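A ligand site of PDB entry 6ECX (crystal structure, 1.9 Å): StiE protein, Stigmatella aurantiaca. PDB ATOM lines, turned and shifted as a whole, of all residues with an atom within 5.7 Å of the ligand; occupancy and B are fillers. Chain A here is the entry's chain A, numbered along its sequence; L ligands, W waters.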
ATOM      1  N   LEU A  19      19.384 -11.117 -23.493  1.00  0.00           N
ATOM      2  CA  LEU A  19      18.341 -12.009 -22.990  1.00  0.00           C
ATOM      3  C   LEU A  19      16.974 -11.355 -23.065  1.00  0.00           C
ATOM      4  O   LEU A  19      15.967 -12.024 -23.343  1.00  0.00           O
ATOM      5  CB  LEU A  19      18.654 -12.419 -21.547  1.00  0.00           C
ATOM      6  CG  LEU A  19      19.843 -13.350 -21.341  1.00  0.00           C
ATOM      7  CD1 LEU A  19      20.165 -13.487 -19.872  1.00  0.00           C
ATOM      8  CD2 LEU A  19      19.555 -14.715 -21.949  1.00  0.00           C
ATOM      9  N   HIS A  36      14.419 -26.392 -22.159  1.00  0.00           N
ATOM     10  CA  HIS A  36      13.753 -26.412 -20.863  1.00  0.00           C
ATOM     11  C   HIS A  36      14.444 -25.495 -19.851  1.00  0.00           C
ATOM     12  O   HIS A  36      13.795 -24.921 -18.975  1.00  0.00           O
ATOM     13  CB  HIS A  36      13.684 -27.838 -20.318  1.00  0.00           C
ATOM     14  CG  HIS A  36      12.533 -28.639 -20.862  1.00  0.00           C
ATOM     15  ND1 HIS A  36      12.595 -30.004 -21.022  1.00  0.00           N
ATOM     16  CD2 HIS A  36      11.299 -28.258 -21.270  1.00  0.00           C
ATOM     17  CE1 HIS A  36      11.439 -30.441 -21.513  1.00  0.00           C
ATOM     18  NE2 HIS A  36      10.634 -29.396 -21.667  1.00  0.00           N
ATOM     19  N   PHE A  37      15.767 -25.363 -19.984  1.00  0.00           N
ATOM     20  CA  PHE A  37      16.580 -24.553 -19.074  1.00  0.00           C
ATOM     21  C   PHE A  37      17.075 -23.302 -19.795  1.00  0.00           C
ATOM     22  O   PHE A  37      17.631 -23.393 -20.891  1.00  0.00           O
ATOM     23  CB  PHE A  37      17.772 -25.359 -18.557  1.00  0.00           C
ATOM     24  CG  PHE A  37      17.448 -26.235 -17.382  1.00  0.00           C
ATOM     25  CD1 PHE A  37      16.679 -25.763 -16.334  1.00  0.00           C
ATOM     26  CD2 PHE A  37      17.919 -27.541 -17.328  1.00  0.00           C
ATOM     27  CE1 PHE A  37      16.392 -26.564 -15.245  1.00  0.00           C
ATOM     28  CE2 PHE A  37      17.631 -28.355 -16.245  1.00  0.00           C
ATOM     29  CZ  PHE A  37      16.861 -27.866 -15.201  1.00  0.00           C
ATOM     30  N   LEU A  38      16.893 -22.135 -19.161  1.00  0.00           N
ATOM     31  CA  LEU A  38      17.335 -20.865 -19.712  1.00  0.00           C
ATOM     32  C   LEU A  38      18.706 -20.426 -19.183  1.00  0.00           C
ATOM     33  O   LEU A  38      19.073 -19.259 -19.321  1.00  0.00           O
ATOM     34  CB  LEU A  38      16.287 -19.780 -19.443  1.00  0.00           C
ATOM     35  CG  LEU A  38      14.943 -20.031 -20.149  1.00  0.00           C
ATOM     36  CD1 LEU A  38      13.920 -18.942 -19.831  1.00  0.00           C
ATOM     37  CD2 LEU A  38      15.133 -20.161 -21.657  1.00  0.00           C
ATOM     38  N   THR A  39      19.449 -21.331 -18.557  1.00  0.00           N
ATOM     39  CA  THR A  39      20.880 -21.190 -18.378  1.00  0.00           C
ATOM     40  C   THR A  39      21.560 -22.273 -19.211  1.00  0.00           C
ATOM     41  O   THR A  39      20.916 -23.242 -19.633  1.00  0.00           O
ATOM     42  CB  THR A  39      21.304 -21.366 -16.913  1.00  0.00           C
ATOM     43  OG1 THR A  39      21.364 -22.762 -16.626  1.00  0.00           O
ATOM     44  CG2 THR A  39      20.312 -20.681 -15.968  1.00  0.00           C
ATOM     45  N   ARG A  77      23.228 -26.996 -12.100  1.00  0.00           N
ATOM     46  CA  ARG A  77      22.288 -27.048 -10.988  1.00  0.00           C
ATOM     47  C   ARG A  77      22.843 -27.850  -9.802  1.00  0.00           C
ATOM     48  O   ARG A  77      22.638 -27.475  -8.637  1.00  0.00           O
ATOM     49  CB  ARG A  77      20.973 -27.665 -11.443  1.00  0.00           C
ATOM     50  CG  ARG A  77      19.859 -26.685 -11.691  1.00  0.00           C
ATOM     51  CD  ARG A  77      20.028 -25.999 -13.013  1.00  0.00           C
ATOM     52  NE  ARG A  77      19.027 -24.963 -13.236  1.00  0.00           N
ATOM     53  CZ  ARG A  77      19.003 -24.192 -14.316  1.00  0.00           C
ATOM     54  NH1 ARG A  77      19.928 -24.358 -15.254  1.00  0.00           N
ATOM     55  NH2 ARG A  77      18.072 -23.262 -14.466  1.00  0.00           N
ATOM     56  N   ASP A  94      11.423 -18.393  -6.276  1.00  0.00           N
ATOM     57  CA  ASP A  94      12.258 -18.213  -7.473  1.00  0.00           C
ATOM     58  C   ASP A  94      11.953 -16.837  -8.040  1.00  0.00           C
ATOM     59  O   ASP A  94      10.877 -16.620  -8.617  1.00  0.00           O
ATOM     60  CB  ASP A  94      11.962 -19.297  -8.515  1.00  0.00           C
ATOM     61  CG  ASP A  94      12.865 -19.194  -9.752  1.00  0.00           C
ATOM     62  OD1 ASP A  94      13.430 -18.113 -10.055  1.00  0.00           O
ATOM     63  OD2 ASP A  94      13.009 -20.233 -10.450  1.00  0.00           O
ATOM     64  N   PHE A  95      12.882 -15.877  -7.876  1.00  0.00           N
ATOM     65  CA  PHE A  95      12.490 -14.518  -8.218  1.00  0.00           C
ATOM     66  C   PHE A  95      12.700 -14.164  -9.683  1.00  0.00           C
ATOM     67  O   PHE A  95      12.491 -13.007 -10.060  1.00  0.00           O
ATOM     68  CB  PHE A  95      13.161 -13.492  -7.283  1.00  0.00           C
ATOM     69  CG  PHE A  95      14.666 -13.454  -7.345  1.00  0.00           C
ATOM     70  CD1 PHE A  95      15.317 -12.679  -8.289  1.00  0.00           C
ATOM     71  CD2 PHE A  95      15.426 -14.101  -6.387  1.00  0.00           C
ATOM     72  CE1 PHE A  95      16.694 -12.587  -8.310  1.00  0.00           C
ATOM     73  CE2 PHE A  95      16.810 -14.003  -6.386  1.00  0.00           C
ATOM     74  CZ  PHE A  95      17.448 -13.258  -7.347  1.00  0.00           C
ATOM     75  N   GLY A  96      13.047 -15.133 -10.528  1.00  0.00           N
ATOM     76  CA  GLY A  96      13.028 -14.927 -11.966  1.00  0.00           C
ATOM     77  C   GLY A  96      12.866 -16.268 -12.643  1.00  0.00           C
ATOM     78  O   GLY A  96      13.826 -16.818 -13.183  1.00  0.00           O
ATOM     79  N   CYS A  97      11.639 -16.821 -12.626  1.00  0.00           N
ATOM     80  CA  CYS A  97      11.458 -18.261 -12.751  1.00  0.00           C
ATOM     81  C   CYS A  97      11.414 -18.785 -14.183  1.00  0.00           C
ATOM     82  O   CYS A  97      11.250 -19.993 -14.365  1.00  0.00           O
ATOM     83  CB  CYS A  97      10.188 -18.688 -11.993  1.00  0.00           C
ATOM     84  SG  CYS A  97       8.637 -17.949 -12.599  1.00  0.00           S
ATOM     85  N   GLY A  98      11.586 -17.932 -15.190  1.00  0.00           N
ATOM     86  CA  GLY A  98      11.695 -18.430 -16.566  1.00  0.00           C
ATOM     87  C   GLY A  98      10.491 -19.273 -16.984  1.00  0.00           C
ATOM     88  O   GLY A  98       9.341 -18.838 -16.888  1.00  0.00           O
ATOM     89  N   HIS A  99      10.770 -20.484 -17.466  1.00  0.00           N
ATOM     90  CA  HIS A  99       9.739 -21.442 -17.861  1.00  0.00           C
ATOM     91  C   HIS A  99       9.383 -22.419 -16.756  1.00  0.00           C
ATOM     92  O   HIS A  99       8.707 -23.422 -17.012  1.00  0.00           O
ATOM     93  CB  HIS A  99      10.169 -22.216 -19.112  1.00  0.00           C
ATOM     94  CG  HIS A  99      10.319 -21.372 -20.338  1.00  0.00           C
ATOM     95  ND1 HIS A  99       9.492 -20.306 -20.599  1.00  0.00           N
ATOM     96  CD2 HIS A  99      11.198 -21.430 -21.367  1.00  0.00           C
ATOM     97  CE1 HIS A  99       9.844 -19.743 -21.738  1.00  0.00           C
ATOM     98  NE2 HIS A  99      10.890 -20.401 -22.223  1.00  0.00           N
ATOM     99  N   ASP A 102      13.042 -25.121 -12.867  1.00  0.00           N
ATOM    100  CA  ASP A 102      13.658 -25.287 -11.543  1.00  0.00           C
ATOM    101  C   ASP A 102      12.607 -25.530 -10.472  1.00  0.00           C
ATOM    102  O   ASP A 102      12.760 -26.434  -9.629  1.00  0.00           O
ATOM    103  CB  ASP A 102      14.498 -24.062 -11.221  1.00  0.00           C
ATOM    104  CG  ASP A 102      15.772 -24.013 -12.037  1.00  0.00           C
ATOM    105  OD1 ASP A 102      16.538 -25.003 -12.018  1.00  0.00           O
ATOM    106  OD2 ASP A 102      16.023 -22.984 -12.707  1.00  0.00           O
ATOM    107  N   TYR A 118       8.165 -15.712  -9.485  1.00  0.00           N
ATOM    108  CA  TYR A 118       7.852 -14.433 -10.117  1.00  0.00           C
ATOM    109  C   TYR A 118       8.574 -14.356 -11.468  1.00  0.00           C
ATOM    110  O   TYR A 118       9.745 -14.725 -11.570  1.00  0.00           O
ATOM    111  CB  TYR A 118       8.327 -13.224  -9.295  1.00  0.00           C
ATOM    112  CG  TYR A 118       7.428 -12.725  -8.169  1.00  0.00           C
ATOM    113  CD1 TYR A 118       6.323 -13.432  -7.758  1.00  0.00           C
ATOM    114  CD2 TYR A 118       7.732 -11.527  -7.514  1.00  0.00           C
ATOM    115  CE1 TYR A 118       5.519 -12.968  -6.744  1.00  0.00           C
ATOM    116  CE2 TYR A 118       6.934 -11.052  -6.488  1.00  0.00           C
ATOM    117  CZ  TYR A 118       5.823 -11.783  -6.116  1.00  0.00           C
ATOM    118  OH  TYR A 118       4.997 -11.338  -5.102  1.00  0.00           O
ATOM    119  N   THR A 119       7.864 -13.870 -12.478  1.00  0.00           N
ATOM    120  CA  THR A 119       8.501 -13.459 -13.726  1.00  0.00           C
ATOM    121  C   THR A 119       7.779 -12.232 -14.245  1.00  0.00           C
ATOM    122  O   THR A 119       6.574 -12.076 -14.028  1.00  0.00           O
ATOM    123  CB  THR A 119       8.468 -14.581 -14.783  1.00  0.00           C
ATOM    124  OG1 THR A 119       9.028 -14.114 -16.017  1.00  0.00           O
ATOM    125  CG2 THR A 119       7.038 -15.037 -15.029  1.00  0.00           C
ATOM    126  N   ILE A 120       8.508 -11.342 -14.919  1.00  0.00           N
ATOM    127  CA  ILE A 120       7.861 -10.155 -15.479  1.00  0.00           C
ATOM    128  C   ILE A 120       7.277 -10.426 -16.846  1.00  0.00           C
ATOM    129  O   ILE A 120       6.500  -9.600 -17.355  1.00  0.00           O
ATOM    130  CB  ILE A 120       8.825  -8.959 -15.579  1.00  0.00           C
ATOM    131  CG1 ILE A 120      10.047  -9.314 -16.419  1.00  0.00           C
ATOM    132  CG2 ILE A 120       9.214  -8.472 -14.190  1.00  0.00           C
ATOM    133  CD1 ILE A 120      11.036  -8.174 -16.536  1.00  0.00           C
ATOM    134  N   SER A 121       7.603 -11.559 -17.473  1.00  0.00           N
ATOM    135  CA  SER A 121       7.055 -11.899 -18.777  1.00  0.00           C
ATOM    136  C   SER A 121       5.680 -12.539 -18.628  1.00  0.00           C
ATOM    137  O   SER A 121       5.550 -13.598 -17.998  1.00  0.00           O
ATOM    138  CB  SER A 121       8.000 -12.839 -19.517  1.00  0.00           C
ATOM    139  OG  SER A 121       7.373 -13.384 -20.665  1.00  0.00           O
ATOM    140  N   GLN A 124       5.850 -15.994 -20.249  1.00  0.00           N
ATOM    141  CA  GLN A 124       6.477 -16.973 -19.374  1.00  0.00           C
ATOM    142  C   GLN A 124       5.535 -17.408 -18.252  1.00  0.00           C
ATOM    143  O   GLN A 124       5.511 -18.577 -17.877  1.00  0.00           O
ATOM    144  CB  GLN A 124       7.767 -16.414 -18.797  1.00  0.00           C
ATOM    145  CG  GLN A 124       8.889 -16.293 -19.835  1.00  0.00           C
ATOM    146  CD  GLN A 124      10.215 -15.847 -19.221  1.00  0.00           C
ATOM    147  OE1 GLN A 124      10.294 -15.516 -18.037  1.00  0.00           O
ATOM    148  NE2 GLN A 124      11.264 -15.833 -20.038  1.00  0.00           N
ATOM    149  N   ARG A 146       5.007 -10.680 -11.794  1.00  0.00           N
ATOM    150  CA  ARG A 146       5.289  -9.598 -10.860  1.00  0.00           C
ATOM    151  C   ARG A 146       6.770  -9.267 -10.944  1.00  0.00           C
ATOM    152  O   ARG A 146       7.593 -10.050 -11.430  1.00  0.00           O
ATOM    153  CB  ARG A 146       4.873  -9.964  -9.428  1.00  0.00           C
ATOM    154  CG  ARG A 146       3.379 -10.294  -9.273  1.00  0.00           C
ATOM    155  CD  ARG A 146       2.741  -9.606  -8.081  1.00  0.00           C
ATOM    156  NE  ARG A 146       2.802 -10.429  -6.898  1.00  0.00           N
ATOM    157  CZ  ARG A 146       1.738 -10.922  -6.257  1.00  0.00           C
ATOM    158  NH1 ARG A 146       0.526 -10.641  -6.686  1.00  0.00           N
ATOM    159  NH2 ARG A 146       1.902 -11.669  -5.184  1.00  0.00           N
ATOM    160  N   ASP A 147       7.110  -8.067 -10.469  1.00  0.00           N
ATOM    161  CA  ASP A 147       8.453  -7.524 -10.563  1.00  0.00           C
ATOM    162  C   ASP A 147       9.119  -7.655  -9.200  1.00  0.00           C
ATOM    163  O   ASP A 147       8.688  -7.022  -8.233  1.00  0.00           O
ATOM    164  CB  ASP A 147       8.406  -6.057 -11.008  1.00  0.00           C
ATOM    165  CG  ASP A 147       9.791  -5.445 -11.216  1.00  0.00           C
ATOM    166  OD1 ASP A 147      10.774  -5.854 -10.541  1.00  0.00           O
ATOM    167  OD2 ASP A 147       9.907  -4.539 -12.062  1.00  0.00           O
ATOM    168  N   SER A 148      10.194  -8.449  -9.151  1.00  0.00           N
ATOM    169  CA  SER A 148      10.852  -8.813  -7.901  1.00  0.00           C
ATOM    170  C   SER A 148      11.524  -7.630  -7.201  1.00  0.00           C
ATOM    171  O   SER A 148      11.866  -7.737  -6.018  1.00  0.00           O
ATOM    172  CB  SER A 148      11.877  -9.918  -8.169  1.00  0.00           C
ATOM    173  OG  SER A 148      11.252 -11.087  -8.647  1.00  0.00           O
ATOM    174  N   ALA A 149      11.737  -6.515  -7.895  1.00  0.00           N
ATOM    175  CA  ALA A 149      12.182  -5.279  -7.264  1.00  0.00           C
ATOM    176  C   ALA A 149      11.033  -4.376  -6.835  1.00  0.00           C
ATOM    177  O   ALA A 149      11.246  -3.472  -6.018  1.00  0.00           O
ATOM    178  CB  ALA A 149      13.106  -4.491  -8.198  1.00  0.00           C
ATOM    179  N   GLY A 162      17.856 -17.385  -7.570  1.00  0.00           N
ATOM    180  CA  GLY A 162      18.008 -16.375  -8.615  1.00  0.00           C
ATOM    181  C   GLY A 162      19.093 -16.806  -9.569  1.00  0.00           C
ATOM    182  O   GLY A 162      20.268 -16.486  -9.350  1.00  0.00           O
ATOM    183  N   PHE A 163      18.741 -17.547 -10.615  1.00  0.00           N
ATOM    184  CA  PHE A 163      19.702 -18.050 -11.584  1.00  0.00           C
ATOM    185  C   PHE A 163      19.656 -17.124 -12.791  1.00  0.00           C
ATOM    186  O   PHE A 163      18.677 -17.123 -13.545  1.00  0.00           O
ATOM    187  CB  PHE A 163      19.417 -19.501 -11.967  1.00  0.00           C
ATOM    188  CG  PHE A 163      19.318 -20.445 -10.772  1.00  0.00           C
ATOM    189  CD1 PHE A 163      19.998 -20.166  -9.580  1.00  0.00           C
ATOM    190  CD2 PHE A 163      18.547 -21.606 -10.850  1.00  0.00           C
ATOM    191  CE1 PHE A 163      19.900 -21.025  -8.489  1.00  0.00           C
ATOM    192  CE2 PHE A 163      18.447 -22.478  -9.763  1.00  0.00           C
ATOM    193  CZ  PHE A 163      19.129 -22.186  -8.567  1.00  0.00           C
ATOM    194  N   GLU A 164      20.694 -16.307 -12.940  1.00  0.00           N
ATOM    195  CA  GLU A 164      20.802 -15.325 -14.024  1.00  0.00           C
ATOM    196  C   GLU A 164      19.610 -14.372 -14.042  1.00  0.00           C
ATOM    197  O   GLU A 164      18.977 -14.148 -15.072  1.00  0.00           O
ATOM    198  CB  GLU A 164      20.974 -16.026 -15.371  1.00  0.00           C
ATOM    199  CG  GLU A 164      22.235 -16.851 -15.521  1.00  0.00           C
ATOM    200  CD  GLU A 164      22.377 -17.447 -16.910  1.00  0.00           C
ATOM    201  OE1 GLU A 164      23.154 -18.409 -17.075  1.00  0.00           O
ATOM    202  OE2 GLU A 164      21.713 -16.949 -17.853  1.00  0.00           O
ATOM    203  N   VAL A 165      19.297 -13.817 -12.866  1.00  0.00           N
ATOM    204  CA  VAL A 165      18.145 -12.918 -12.727  1.00  0.00           C
ATOM    205  C   VAL A 165      18.580 -11.583 -12.148  1.00  0.00           C
ATOM    206  O   VAL A 165      18.303 -10.520 -12.723  1.00  0.00           O
ATOM    207  CB  VAL A 165      17.055 -13.555 -11.838  1.00  0.00           C
ATOM    208  CG1 VAL A 165      15.845 -12.624 -11.780  1.00  0.00           C
ATOM    209  CG2 VAL A 165      16.679 -14.938 -12.333  1.00  0.00           C
ATOM    210  N   LEU A 168      19.845  -8.731 -14.175  1.00  0.00           N
ATOM    211  CA  LEU A 168      18.914  -8.088 -15.086  1.00  0.00           C
ATOM    212  C   LEU A 168      18.067  -7.006 -14.430  1.00  0.00           C
ATOM    213  O   LEU A 168      17.299  -6.329 -15.129  1.00  0.00           O
ATOM    214  CB  LEU A 168      17.965  -9.141 -15.678  1.00  0.00           C
ATOM    215  CG  LEU A 168      18.383  -9.975 -16.878  1.00  0.00           C
ATOM    216  CD1 LEU A 168      17.547 -11.243 -16.949  1.00  0.00           C
ATOM    217  CD2 LEU A 168      18.219  -9.174 -18.145  1.00  0.00           C
ATOM    218  N   ILE A 169      18.155  -6.860 -13.114  1.00  0.00           N
ATOM    219  CA  ILE A 169      17.232  -6.046 -12.337  1.00  0.00           C
ATOM    220  C   ILE A 169      17.964  -4.774 -11.916  1.00  0.00           C
ATOM    221  O   ILE A 169      18.923  -4.841 -11.134  1.00  0.00           O
ATOM    222  CB  ILE A 169      16.691  -6.817 -11.117  1.00  0.00           C
ATOM    223  CG1 ILE A 169      15.821  -7.984 -11.609  1.00  0.00           C
ATOM    224  CG2 ILE A 169      15.892  -5.884 -10.218  1.00  0.00           C
ATOM    225  CD1 ILE A 169      15.231  -8.867 -10.512  1.00  0.00           C
HETATM  226  N1  LIG L   1      15.951 -18.695 -13.738  1.00  0.00           N
HETATM  227  C1  LIG L   1      15.415 -19.194 -14.991  1.00  0.00           C
HETATM  228  C2  LIG L   1      16.297 -20.298 -15.567  1.00  0.00           C
HETATM  229  O1  LIG L   1      17.413 -20.472 -15.089  1.00  0.00           O
HETATM  230  O2  LIG L   1      15.923 -21.041 -16.482  1.00  0.00           O
HETATM  231  C3  LIG L   1      15.281 -18.062 -15.994  1.00  0.00           C
HETATM  232  C4  LIG L   1      16.534 -17.214 -16.173  1.00  0.00           C
HETATM  233  S1  LIG L   1      16.308 -16.035 -17.529  1.00  0.00           S
HETATM  234  C5  LIG L   1      18.007 -15.883 -18.131  1.00  0.00           C
HETATM  235  C6  LIG L   1      15.953 -14.492 -16.657  1.00  0.00           C
HETATM  236  C7  LIG L   1      14.569 -14.485 -16.006  1.00  0.00           C
HETATM  237  O3  LIG L   1      14.404 -13.416 -15.089  1.00  0.00           O
HETATM  238  C8  LIG L   1      13.389 -14.372 -16.974  1.00  0.00           C
HETATM  239  O4  LIG L   1      12.444 -15.344 -16.556  1.00  0.00           O
HETATM  240  C9  LIG L   1      12.808 -12.982 -16.715  1.00  0.00           C
HETATM  241  O5  LIG L   1      11.414 -12.897 -16.915  1.00  0.00           O
HETATM  242  C10 LIG L   1      13.124 -12.815 -15.236  1.00  0.00           C
HETATM  243  N2  LIG L   1      13.162 -11.431 -14.724  1.00  0.00           N
HETATM  244  C11 LIG L   1      13.950 -10.408 -15.203  1.00  0.00           C
HETATM  245  N3  LIG L   1      13.720  -9.302 -14.452  1.00  0.00           N
HETATM  246  C12 LIG L   1      12.797  -9.600 -13.511  1.00  0.00           C
HETATM  247  C13 LIG L   1      12.211  -8.854 -12.496  1.00  0.00           C
HETATM  248  N4  LIG L   1      12.536  -7.572 -12.321  1.00  0.00           N
HETATM  249  N5  LIG L   1      11.283  -9.446 -11.658  1.00  0.00           N
HETATM  250  C14 LIG L   1      10.940 -10.768 -11.819  1.00  0.00           C
HETATM  251  N6  LIG L   1      11.538 -11.497 -12.822  1.00  0.00           N
HETATM  252  C15 LIG L   1      12.443 -10.938 -13.663  1.00  0.00           C
HETATM  253  O   HOH W   1      13.628 -22.473 -14.307  1.00  0.00           O
HETATM  254  O   HOH W   2      13.253 -22.076 -17.140  1.00  0.00           O
HETATM  255  O   HOH W   3      14.357  -6.640 -14.944  1.00  0.00           O
HETATM  256  O   HOH W   4      16.046 -18.420 -10.671  1.00  0.00           O
HETATM  257  O   HOH W   5      15.239 -20.750 -12.055  1.00  0.00           O
HETATM  258  O   HOH W   6      12.838  -4.540 -12.175  1.00  0.00           O
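The backbone carbonyl oxygen of Phe 95 lies close to a nitrogen (N6) of the ligand, at 3.3 Å.
Merely in contact with the ligand: Leu 19 (3.7 Å), Thr 39 (3.0 Å), Asp 102 (3.7 Å), Tyr 118 (3.9 Å), Ile 120 (3.4 Å), Arg 146 (3.4 Å), Glu 164 (3.4 Å), Val 165 (3.7 Å), Leu 168 (3.6 Å) and Ile 169 (3.4 Å).
Hydrophobic or aromatic side chains within 4 Å of the ligand: Leu 19, Leu 38, Ile 120, Phe 163, Val 165, Leu 168 and Ile 169.
The nearest printed residue that does not touch the ligand is Ser 121 (4.1 Å).
Water W5 lies within hydrogen-bond range of OD2 of Asp 102 (2.5 Å), N1 of the ligand (2.7 Å) and OD2 of Asp 94 (2.8 Å).
Water W3 bridges N3 of the ligand (2.8 Å) and O of Leu 168 (3.0 Å).
Water W2 lies within hydrogen-bond range of O2 of the ligand (2.9 Å), N of His 99 (3.0 Å) and O of His 36 (3.4 Å).
Water W6 bridges OD2 of Asp 147 (2.9 Å) and N4 of the ligand (3.1 Å).
Water W4 lies within hydrogen-bond range of the side-chain carboxylate of Asp 94 (2.7 Å), the backbone NH of Phe 163 (2.8 Å) and a nitrogen (N1) of the ligand (3.1 Å).
Water W1 lies within hydrogen-bond range of the side-chain carboxylate of Asp 102, the backbone carbonyl oxygen of Cys 97 and an oxygen (O2) of the ligand.
OE1 of Gln 124 is in hydrogen-bond range of O4 of the ligand (2.6 Å).
OG1 of Thr 119 sits at hydrogen-bond distance from O5 of the ligand.
O of Gly 96 is in hydrogen-bond range of N1 of the ligand (2.9 Å).
The backbone NH of Ser 148 lies within hydrogen-bond range of a nitrogen (N5) of the ligand.
A nitrogen (N5) of the ligand sits close to the side-chain hydroxyl (OG) of Ser 148, at 3.4 Å.
The guanidinium group of Arg 77 is in salt-bridge range of an oxygen (O1) of the ligand, 2.9 Å away.
N4 of the ligand sits at hydrogen-bond distance from OD1 of Asp 147 (3.0 Å).
The backbone NH (N) of Gly 98 is in hydrogen-bond range of an oxygen (O4) of the ligand, at 3.0 Å.
The backbone NH of Leu 38 is in hydrogen-bond range of an oxygen (O2) of the ligand, at 3.1 Å.
O of Phe 163 lies within hydrogen-bond range of N1 of the ligand (3.2 Å).
OG of Ser 121 is in hydrogen-bond range of N of Gln 124 (3.1 Å).
The backbone carbonyl oxygen of Thr 119 is in hydrogen-bond range of the backbone NH of Arg 146.
The side-chain hydroxyl (OG1) of Thr 119 is in hydrogen-bond range of the backbone NH (N) of Ser 121 (3.3 Å).
The backbone carbonyl oxygen of Tyr 118 lies close to the backbone NH of Gly 96 (3.5 Å).
The side-chain hydroxyl of Ser 148 sits at hydrogen-bond distance from the backbone carbonyl oxygen of Phe 95 (2.7 Å).
The guanidinium group (NH2) of Arg 77 is in salt-bridge range of the side-chain carboxylate (OD2) of Asp 102, at 2.7 Å.
The side-chain carboxylate (OD1) of Asp 147 is in hydrogen-bond range of the backbone NH (N) of Ala 149.
OH of Tyr 118 is in hydrogen-bond range of NE of Arg 146.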
